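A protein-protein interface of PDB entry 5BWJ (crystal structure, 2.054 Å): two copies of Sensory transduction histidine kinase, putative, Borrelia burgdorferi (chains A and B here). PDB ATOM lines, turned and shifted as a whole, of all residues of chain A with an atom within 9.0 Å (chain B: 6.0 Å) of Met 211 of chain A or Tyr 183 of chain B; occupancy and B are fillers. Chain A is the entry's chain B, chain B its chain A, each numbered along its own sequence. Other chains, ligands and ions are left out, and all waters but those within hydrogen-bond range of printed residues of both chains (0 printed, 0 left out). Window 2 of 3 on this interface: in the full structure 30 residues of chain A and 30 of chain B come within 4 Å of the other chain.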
ATOM      1  N   PRO A  18     -22.417 -31.352  13.140  1.00  0.00           N
ATOM      2  CA  PRO A  18     -23.131 -30.236  13.774  1.00  0.00           C
ATOM      3  C   PRO A  18     -22.386 -28.902  13.680  1.00  0.00           C
ATOM      4  O   PRO A  18     -22.739 -27.956  14.384  1.00  0.00           O
ATOM      5  CB  PRO A  18     -23.223 -30.689  15.228  1.00  0.00           C
ATOM      6  CG  PRO A  18     -21.916 -31.394  15.443  1.00  0.00           C
ATOM      7  CD  PRO A  18     -21.561 -32.050  14.119  1.00  0.00           C
ATOM      8  N   PHE A  19     -21.363 -28.833  12.836  1.00  0.00           N
ATOM      9  CA  PHE A  19     -20.547 -27.626  12.728  1.00  0.00           C
ATOM     10  C   PHE A  19     -21.323 -26.471  12.103  1.00  0.00           C
ATOM     11  O   PHE A  19     -21.258 -25.342  12.586  1.00  0.00           O
ATOM     12  CB  PHE A  19     -19.279 -27.919  11.925  1.00  0.00           C
ATOM     13  CG  PHE A  19     -18.335 -28.851  12.627  1.00  0.00           C
ATOM     14  CD1 PHE A  19     -17.345 -28.355  13.459  1.00  0.00           C
ATOM     15  CD2 PHE A  19     -18.453 -30.222  12.474  1.00  0.00           C
ATOM     16  CE1 PHE A  19     -16.482 -29.210  14.114  1.00  0.00           C
ATOM     17  CE2 PHE A  19     -17.594 -31.082  13.128  1.00  0.00           C
ATOM     18  CZ  PHE A  19     -16.607 -30.575  13.950  1.00  0.00           C
ATOM     19  N   LEU A  31     -21.906 -24.967  15.673  1.00  0.00           N
ATOM     20  CA  LEU A  31     -20.923 -24.625  16.694  1.00  0.00           C
ATOM     21  C   LEU A  31     -19.617 -24.100  16.095  1.00  0.00           C
ATOM     22  O   LEU A  31     -18.716 -23.698  16.832  1.00  0.00           O
ATOM     23  CB  LEU A  31     -20.639 -25.849  17.574  1.00  0.00           C
ATOM     24  CG  LEU A  31     -20.200 -27.133  16.863  1.00  0.00           C
ATOM     25  CD1 LEU A  31     -18.695 -27.180  16.685  1.00  0.00           C
ATOM     26  CD2 LEU A  31     -20.684 -28.354  17.623  1.00  0.00           C
ATOM     27  N   ILE A  35     -16.134 -21.802  17.502  1.00  0.00           N
ATOM     28  CA  ILE A  35     -14.757 -22.245  17.321  1.00  0.00           C
ATOM     29  C   ILE A  35     -13.923 -21.194  16.594  1.00  0.00           C
ATOM     30  O   ILE A  35     -12.784 -20.927  16.973  1.00  0.00           O
ATOM     31  CB  ILE A  35     -14.687 -23.566  16.526  1.00  0.00           C
ATOM     32  CG1 ILE A  35     -15.464 -24.668  17.249  1.00  0.00           C
ATOM     33  CG2 ILE A  35     -13.233 -24.001  16.328  1.00  0.00           C
ATOM     34  CD1 ILE A  35     -15.648 -25.925  16.424  1.00  0.00           C
ATOM     35  N   LYS A  38     -12.915 -18.282  18.680  1.00  0.00           N
ATOM     36  CA  LYS A  38     -11.818 -18.655  19.565  1.00  0.00           C
ATOM     37  C   LYS A  38     -10.492 -18.636  18.813  1.00  0.00           C
ATOM     38  O   LYS A  38      -9.508 -18.064  19.287  1.00  0.00           O
ATOM     39  CB  LYS A  38     -12.054 -20.038  20.175  1.00  0.00           C
ATOM     40  CG  LYS A  38     -13.073 -20.059  21.300  1.00  0.00           C
ATOM     41  CD  LYS A  38     -13.031 -21.381  22.044  1.00  0.00           C
ATOM     42  CE  LYS A  38     -13.821 -21.318  23.336  1.00  0.00           C
ATOM     43  NZ  LYS A  38     -13.549 -22.500  24.196  1.00  0.00           N
ATOM     44  N   LEU A 206      -8.273 -25.931  13.808  1.00  0.00           N
ATOM     45  CA  LEU A 206      -9.508 -25.515  14.462  1.00  0.00           C
ATOM     46  C   LEU A 206      -9.972 -26.553  15.476  1.00  0.00           C
ATOM     47  O   LEU A 206     -10.600 -26.215  16.478  1.00  0.00           O
ATOM     48  CB  LEU A 206     -10.606 -25.274  13.421  1.00  0.00           C
ATOM     49  CG  LEU A 206     -10.287 -24.240  12.340  1.00  0.00           C
ATOM     50  CD1 LEU A 206     -11.418 -24.170  11.321  1.00  0.00           C
ATOM     51  CD2 LEU A 206     -10.034 -22.869  12.950  1.00  0.00           C
ATOM     52  N   PHE A 207      -9.654 -27.816  15.217  1.00  0.00           N
ATOM     53  CA  PHE A 207     -10.080 -28.908  16.085  1.00  0.00           C
ATOM     54  C   PHE A 207      -9.494 -28.786  17.489  1.00  0.00           C
ATOM     55  O   PHE A 207     -10.113 -29.210  18.464  1.00  0.00           O
ATOM     56  CB  PHE A 207      -9.688 -30.255  15.475  1.00  0.00           C
ATOM     57  CG  PHE A 207     -10.023 -31.432  16.347  1.00  0.00           C
ATOM     58  CD1 PHE A 207     -11.305 -31.954  16.366  1.00  0.00           C
ATOM     59  CD2 PHE A 207      -9.055 -32.017  17.146  1.00  0.00           C
ATOM     60  CE1 PHE A 207     -11.617 -33.037  17.166  1.00  0.00           C
ATOM     61  CE2 PHE A 207      -9.360 -33.101  17.950  1.00  0.00           C
ATOM     62  CZ  PHE A 207     -10.643 -33.611  17.960  1.00  0.00           C
ATOM     63  N   SER A 208      -8.304 -28.204  17.592  1.00  0.00           N
ATOM     64  CA  SER A 208      -7.637 -28.065  18.881  1.00  0.00           C
ATOM     65  C   SER A 208      -8.432 -27.165  19.825  1.00  0.00           C
ATOM     66  O   SER A 208      -8.332 -27.295  21.046  1.00  0.00           O
ATOM     67  CB  SER A 208      -6.224 -27.507  18.697  1.00  0.00           C
ATOM     68  OG  SER A 208      -6.260 -26.178  18.210  1.00  0.00           O
ATOM     69  N   TYR A 209      -9.223 -26.258  19.258  1.00  0.00           N
ATOM     70  CA  TYR A 209     -10.023 -25.336  20.057  1.00  0.00           C
ATOM     71  C   TYR A 209     -11.267 -26.016  20.623  1.00  0.00           C
ATOM     72  O   TYR A 209     -12.045 -25.402  21.355  1.00  0.00           O
ATOM     73  CB  TYR A 209     -10.405 -24.114  19.221  1.00  0.00           C
ATOM     74  CG  TYR A 209      -9.205 -23.270  18.873  1.00  0.00           C
ATOM     75  CD1 TYR A 209      -8.857 -22.173  19.648  1.00  0.00           C
ATOM     76  CD2 TYR A 209      -8.398 -23.588  17.789  1.00  0.00           C
ATOM     77  CE1 TYR A 209      -7.752 -21.406  19.343  1.00  0.00           C
ATOM     78  CE2 TYR A 209      -7.287 -22.827  17.476  1.00  0.00           C
ATOM     79  CZ  TYR A 209      -6.969 -21.738  18.257  1.00  0.00           C
ATOM     80  OH  TYR A 209      -5.865 -20.977  17.951  1.00  0.00           O
ATOM     81  N   LEU A 210     -11.447 -27.285  20.273  1.00  0.00           N
ATOM     82  CA  LEU A 210     -12.403 -28.147  20.952  1.00  0.00           C
ATOM     83  C   LEU A 210     -11.670 -28.871  22.071  1.00  0.00           C
ATOM     84  O   LEU A 210     -10.952 -29.842  21.828  1.00  0.00           O
ATOM     85  CB  LEU A 210     -13.036 -29.145  19.978  1.00  0.00           C
ATOM     86  CG  LEU A 210     -14.476 -28.889  19.524  1.00  0.00           C
ATOM     87  CD1 LEU A 210     -14.723 -27.434  19.167  1.00  0.00           C
ATOM     88  CD2 LEU A 210     -14.802 -29.785  18.337  1.00  0.00           C
ATOM     89  N   MET A 211     -11.837 -28.374  23.294  1.00  0.00           N
ATOM     90  CA  MET A 211     -11.152 -28.928  24.455  1.00  0.00           C
ATOM     91  C   MET A 211     -11.418 -30.424  24.578  1.00  0.00           C
ATOM     92  O   MET A 211     -12.559 -30.873  24.472  1.00  0.00           O
ATOM     93  CB  MET A 211     -11.595 -28.207  25.729  1.00  0.00           C
ATOM     94  N   LYS A 212     -10.352 -31.191  24.792  1.00  0.00           N
ATOM     95  CA  LYS A 212     -10.452 -32.642  24.861  1.00  0.00           C
ATOM     96  C   LYS A 212     -10.735 -33.104  26.286  1.00  0.00           C
ATOM     97  O   LYS A 212     -10.582 -32.342  27.240  1.00  0.00           O
ATOM     98  CB  LYS A 212      -9.166 -33.290  24.346  1.00  0.00           C
ATOM     99  N   MET A 213     -11.153 -34.360  26.415  1.00  0.00           N
ATOM    100  CA  MET A 213     -11.444 -34.949  27.717  1.00  0.00           C
ATOM    101  C   MET A 213     -10.163 -35.359  28.437  1.00  0.00           C
ATOM    102  O   MET A 213      -9.528 -36.346  28.064  1.00  0.00           O
ATOM    103  CB  MET A 213     -12.359 -36.162  27.554  1.00  0.00           C
ATOM    104  N   PRO A 214      -9.785 -34.599  29.476  1.00  0.00           N
ATOM    105  CA  PRO A 214      -8.592 -34.823  30.301  1.00  0.00           C
ATOM    106  C   PRO A 214      -7.315 -34.961  29.474  1.00  0.00           C
ATOM    107  O   PRO A 214      -6.765 -33.945  29.049  1.00  0.00           O
ATOM    108  CB  PRO A 214      -8.913 -36.130  31.032  1.00  0.00           C
ATOM    109  N   SER B  88     -17.564 -37.935  19.113  1.00  0.00           N
ATOM    110  CA  SER B  88     -18.749 -37.091  19.196  1.00  0.00           C
ATOM    111  C   SER B  88     -18.366 -35.707  19.693  1.00  0.00           C
ATOM    112  O   SER B  88     -17.227 -35.477  20.105  1.00  0.00           O
ATOM    113  CB  SER B  88     -19.797 -37.710  20.125  1.00  0.00           C
ATOM    114  OG  SER B  88     -20.285 -38.935  19.609  1.00  0.00           O
ATOM    115  N   ILE B  89     -19.326 -34.791  19.646  1.00  0.00           N
ATOM    116  CA  ILE B  89     -19.154 -33.459  20.204  1.00  0.00           C
ATOM    117  C   ILE B  89     -20.284 -33.193  21.189  1.00  0.00           C
ATOM    118  O   ILE B  89     -21.452 -33.431  20.890  1.00  0.00           O
ATOM    119  CB  ILE B  89     -19.131 -32.381  19.103  1.00  0.00           C
ATOM    120  CG1 ILE B  89     -17.934 -32.617  18.176  1.00  0.00           C
ATOM    121  CG2 ILE B  89     -19.062 -30.981  19.718  1.00  0.00           C
ATOM    122  CD1 ILE B  89     -17.889 -31.703  16.963  1.00  0.00           C
ATOM    123  N   SER B  90     -19.922 -32.724  22.377  1.00  0.00           N
ATOM    124  CA  SER B  90     -20.905 -32.383  23.396  1.00  0.00           C
ATOM    125  C   SER B  90     -21.646 -31.106  23.012  1.00  0.00           C
ATOM    126  O   SER B  90     -21.023 -30.101  22.668  1.00  0.00           O
ATOM    127  CB  SER B  90     -20.230 -32.216  24.759  1.00  0.00           C
ATOM    128  OG  SER B  90     -19.240 -31.202  24.717  1.00  0.00           O
ATOM    129  N   ILE B 125     -18.623 -33.327  33.002  1.00  0.00           N
ATOM    130  CA  ILE B 125     -18.363 -31.999  32.458  1.00  0.00           C
ATOM    131  C   ILE B 125     -19.215 -30.961  33.182  1.00  0.00           C
ATOM    132  O   ILE B 125     -18.712 -29.917  33.596  1.00  0.00           O
ATOM    133  CB  ILE B 125     -18.635 -31.952  30.937  1.00  0.00           C
ATOM    134  CG1 ILE B 125     -17.533 -32.710  30.194  1.00  0.00           C
ATOM    135  CG2 ILE B 125     -18.699 -30.505  30.425  1.00  0.00           C
ATOM    136  CD1 ILE B 125     -17.840 -32.983  28.735  1.00  0.00           C
ATOM    137  N   LEU B 128     -17.904 -30.524  36.862  1.00  0.00           N
ATOM    138  CA  LEU B 128     -16.673 -29.752  37.025  1.00  0.00           C
ATOM    139  C   LEU B 128     -16.885 -28.292  36.628  1.00  0.00           C
ATOM    140  O   LEU B 128     -16.081 -27.427  36.976  1.00  0.00           O
ATOM    141  CB  LEU B 128     -15.524 -30.372  36.217  1.00  0.00           C
ATOM    142  CG  LEU B 128     -15.597 -30.413  34.688  1.00  0.00           C
ATOM    143  CD1 LEU B 128     -15.044 -29.138  34.059  1.00  0.00           C
ATOM    144  CD2 LEU B 128     -14.848 -31.634  34.164  1.00  0.00           C
ATOM    145  N   LYS B 129     -17.969 -28.024  35.903  1.00  0.00           N
ATOM    146  CA  LYS B 129     -18.376 -26.655  35.596  1.00  0.00           C
ATOM    147  C   LYS B 129     -19.220 -26.073  36.729  1.00  0.00           C
ATOM    148  O   LYS B 129     -19.729 -24.957  36.623  1.00  0.00           O
ATOM    149  CB  LYS B 129     -19.162 -26.605  34.284  1.00  0.00           C
ATOM    150  CG  LYS B 129     -18.305 -26.710  33.032  1.00  0.00           C
ATOM    151  CD  LYS B 129     -19.166 -26.672  31.776  1.00  0.00           C
ATOM    152  CE  LYS B 129     -18.320 -26.649  30.514  1.00  0.00           C
ATOM    153  NZ  LYS B 129     -17.521 -25.396  30.393  1.00  0.00           N
ATOM    154  N   TYR B 156     -27.901 -31.867  27.755  1.00  0.00           N
ATOM    155  CA  TYR B 156     -26.488 -31.898  27.400  1.00  0.00           C
ATOM    156  C   TYR B 156     -26.070 -33.320  27.044  1.00  0.00           C
ATOM    157  O   TYR B 156     -26.293 -34.246  27.824  1.00  0.00           O
ATOM    158  CB  TYR B 156     -25.653 -31.365  28.567  1.00  0.00           C
ATOM    159  CG  TYR B 156     -24.214 -31.043  28.240  1.00  0.00           C
ATOM    160  CD1 TYR B 156     -23.891 -30.122  27.251  1.00  0.00           C
ATOM    161  CD2 TYR B 156     -23.177 -31.635  28.945  1.00  0.00           C
ATOM    162  CE1 TYR B 156     -22.576 -29.818  26.961  1.00  0.00           C
ATOM    163  CE2 TYR B 156     -21.860 -31.336  28.665  1.00  0.00           C
ATOM    164  CZ  TYR B 156     -21.564 -30.426  27.673  1.00  0.00           C
ATOM    165  OH  TYR B 156     -20.250 -30.125  27.390  1.00  0.00           O
ATOM    166  N   ASP B 180     -19.271 -21.906  25.860  1.00  0.00           N
ATOM    167  CA  ASP B 180     -18.106 -22.765  26.034  1.00  0.00           C
ATOM    168  C   ASP B 180     -18.523 -24.116  26.613  1.00  0.00           C
ATOM    169  O   ASP B 180     -18.181 -24.453  27.748  1.00  0.00           O
ATOM    170  CB  ASP B 180     -17.069 -22.087  26.935  1.00  0.00           C
ATOM    171  CG  ASP B 180     -15.804 -22.911  27.093  1.00  0.00           C
ATOM    172  OD1 ASP B 180     -15.093 -23.111  26.085  1.00  0.00           O
ATOM    173  OD2 ASP B 180     -15.517 -23.354  28.225  1.00  0.00           O
ATOM    174  N   VAL B 181     -19.266 -24.883  25.819  1.00  0.00           N
ATOM    175  CA  VAL B 181     -19.785 -26.179  26.245  1.00  0.00           C
ATOM    176  C   VAL B 181     -19.435 -27.281  25.249  1.00  0.00           C
ATOM    177  O   VAL B 181     -19.844 -28.432  25.419  1.00  0.00           O
ATOM    178  CB  VAL B 181     -21.320 -26.136  26.420  1.00  0.00           C
ATOM    179  CG1 VAL B 181     -21.700 -25.171  27.531  1.00  0.00           C
ATOM    180  CG2 VAL B 181     -21.998 -25.739  25.114  1.00  0.00           C
ATOM    181  N   PHE B 182     -18.683 -26.925  24.211  1.00  0.00           N
ATOM    182  CA  PHE B 182     -18.345 -27.869  23.153  1.00  0.00           C
ATOM    183  C   PHE B 182     -17.021 -28.552  23.439  1.00  0.00           C
ATOM    184  O   PHE B 182     -15.985 -27.896  23.549  1.00  0.00           O
ATOM    185  CB  PHE B 182     -18.280 -27.164  21.798  1.00  0.00           C
ATOM    186  CG  PHE B 182     -19.505 -26.364  21.478  1.00  0.00           C
ATOM    187  CD1 PHE B 182     -20.718 -26.990  21.253  1.00  0.00           C
ATOM    188  CD2 PHE B 182     -19.443 -24.984  21.398  1.00  0.00           C
ATOM    189  CE1 PHE B 182     -21.851 -26.253  20.958  1.00  0.00           C
ATOM    190  CE2 PHE B 182     -20.571 -24.242  21.103  1.00  0.00           C
ATOM    191  CZ  PHE B 182     -21.776 -24.878  20.884  1.00  0.00           C
ATOM    192  N   TYR B 183     -17.069 -29.876  23.560  1.00  0.00           N
ATOM    193  CA  TYR B 183     -15.874 -30.679  23.781  1.00  0.00           C
ATOM    194  C   TYR B 183     -15.860 -31.877  22.841  1.00  0.00           C
ATOM    195  O   TYR B 183     -16.907 -32.439  22.522  1.00  0.00           O
ATOM    196  CB  TYR B 183     -15.807 -31.152  25.236  1.00  0.00           C
ATOM    197  CG  TYR B 183     -15.750 -30.028  26.246  1.00  0.00           C
ATOM    198  CD1 TYR B 183     -14.570 -29.333  26.474  1.00  0.00           C
ATOM    199  CD2 TYR B 183     -16.873 -29.668  26.976  1.00  0.00           C
ATOM    200  CE1 TYR B 183     -14.511 -28.307  27.398  1.00  0.00           C
ATOM    201  CE2 TYR B 183     -16.825 -28.644  27.903  1.00  0.00           C
ATOM    202  CZ  TYR B 183     -15.641 -27.967  28.111  1.00  0.00           C
ATOM    203  OH  TYR B 183     -15.586 -26.945  29.031  1.00  0.00           O
ATOM    204  N   SER B 184     -14.668 -32.254  22.392  1.00  0.00           N
ATOM    205  CA  SER B 184     -14.500 -33.465  21.602  1.00  0.00           C
ATOM    206  C   SER B 184     -14.593 -34.683  22.517  1.00  0.00           C
ATOM    207  O   SER B 184     -13.822 -34.805  23.467  1.00  0.00           O
ATOM    208  CB  SER B 184     -13.161 -33.451  20.864  1.00  0.00           C
ATOM    209  OG  SER B 184     -12.966 -34.655  20.141  1.00  0.00           O
ATOM    210  N   ILE B 185     -15.541 -35.570  22.229  1.00  0.00           N
ATOM    211  CA  ILE B 185     -15.805 -36.736  23.070  1.00  0.00           C
ATOM    212  C   ILE B 185     -15.410 -38.031  22.366  1.00  0.00           C
ATOM    213  O   ILE B 185     -15.828 -38.286  21.238  1.00  0.00           O
ATOM    214  CB  ILE B 185     -17.299 -36.823  23.459  1.00  0.00           C
ATOM    215  CG1 ILE B 185     -17.771 -35.516  24.105  1.00  0.00           C
ATOM    216  CG2 ILE B 185     -17.547 -38.004  24.393  1.00  0.00           C
ATOM    217  CD1 ILE B 185     -17.030 -35.138  25.376  1.00  0.00           C
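Phe 19 of chain A touches Ile 89 of chain B.
CG2 of Ile 89 of chain B touches CD2 of Leu 31 of chain A, 3.7 Å away.
Phe 182 of chain B touches Leu 31 of chain A.
CZ of Phe 207 of chain A touches OG of Ser 184 of chain B, at 3.4 Å.
Leu 210 of chain A touches Ile 89 of chain B (CD2 to CD1, 3.9 Å).
Met 211 of chain A touches Tyr 183 of chain B (O to CD1, 3.2 Å).
The side-chain hydroxyl (OG) of Ser 90 of chain B lies within hydrogen-bond range of the backbone NH (N) of Tyr 183 of chain B, at 2.8 Å.
The side-chain carboxylate (OD2) of Asp 180 of chain B is in salt-bridge range of the side-chain amino group (NZ) of Lys 129 of chain B, 3.6 Å away.
The side-chain amino group of Lys 129 of chain B lies within hydrogen-bond range of the side-chain hydroxyl of Tyr 183 of chain B.
The backbone carbonyl oxygen (O) of Pro 18 of chain A sits at hydrogen-bond distance from the backbone NH (N) of Leu 31 of chain A (3.4 Å).
The backbone carbonyl oxygen (O) of Phe 19 of chain A is in hydrogen-bond range of the backbone NH (N) of Leu 31 of chain A (3.2 Å).
Printed residues of chain B that touch a printed residue of chain A: Ile 89, Asp 180, Phe 182, Tyr 183 and Ser 184.
Of the 14 printed residues of chain A, 6 touch a printed residue of chain B.
Along chain A the printed residues that touch a printed residue of chain B span positions 19 to 211.
Among the printed residues, 8 pairs touch across the chains.
The side-chain carboxylate (OD1) of Asp 180 of chain B lies within salt-bridge range of the side-chain amino group (NZ) of Lys 38 of chain A (2.5 Å).
The backbone NH of Ser 184 of chain B lies within hydrogen-bond range of the backbone carbonyl oxygen of Met 211 of chain A.
No position is printed for both chains.
Of the 8 pairs that touch across the chains among the printed residues, none has its exchanged pair printed and touching as well.
Met 211 of chain A touches just these residues of chain B: Tyr 183 and Ser 184.
Tyr 183 of chain B touches just one residue of chain A: Met 211.
No residue of chain A comes within 4 Å of Ser 90 of chain B.
Of the printed residues of chain B, Phe 19 of chain A touches Ile 89.
Of the printed residues of chain B, Lys 38 of chain A touches Asp 180.
Pro 214 of chain A touches none of the printed residues of chain B.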
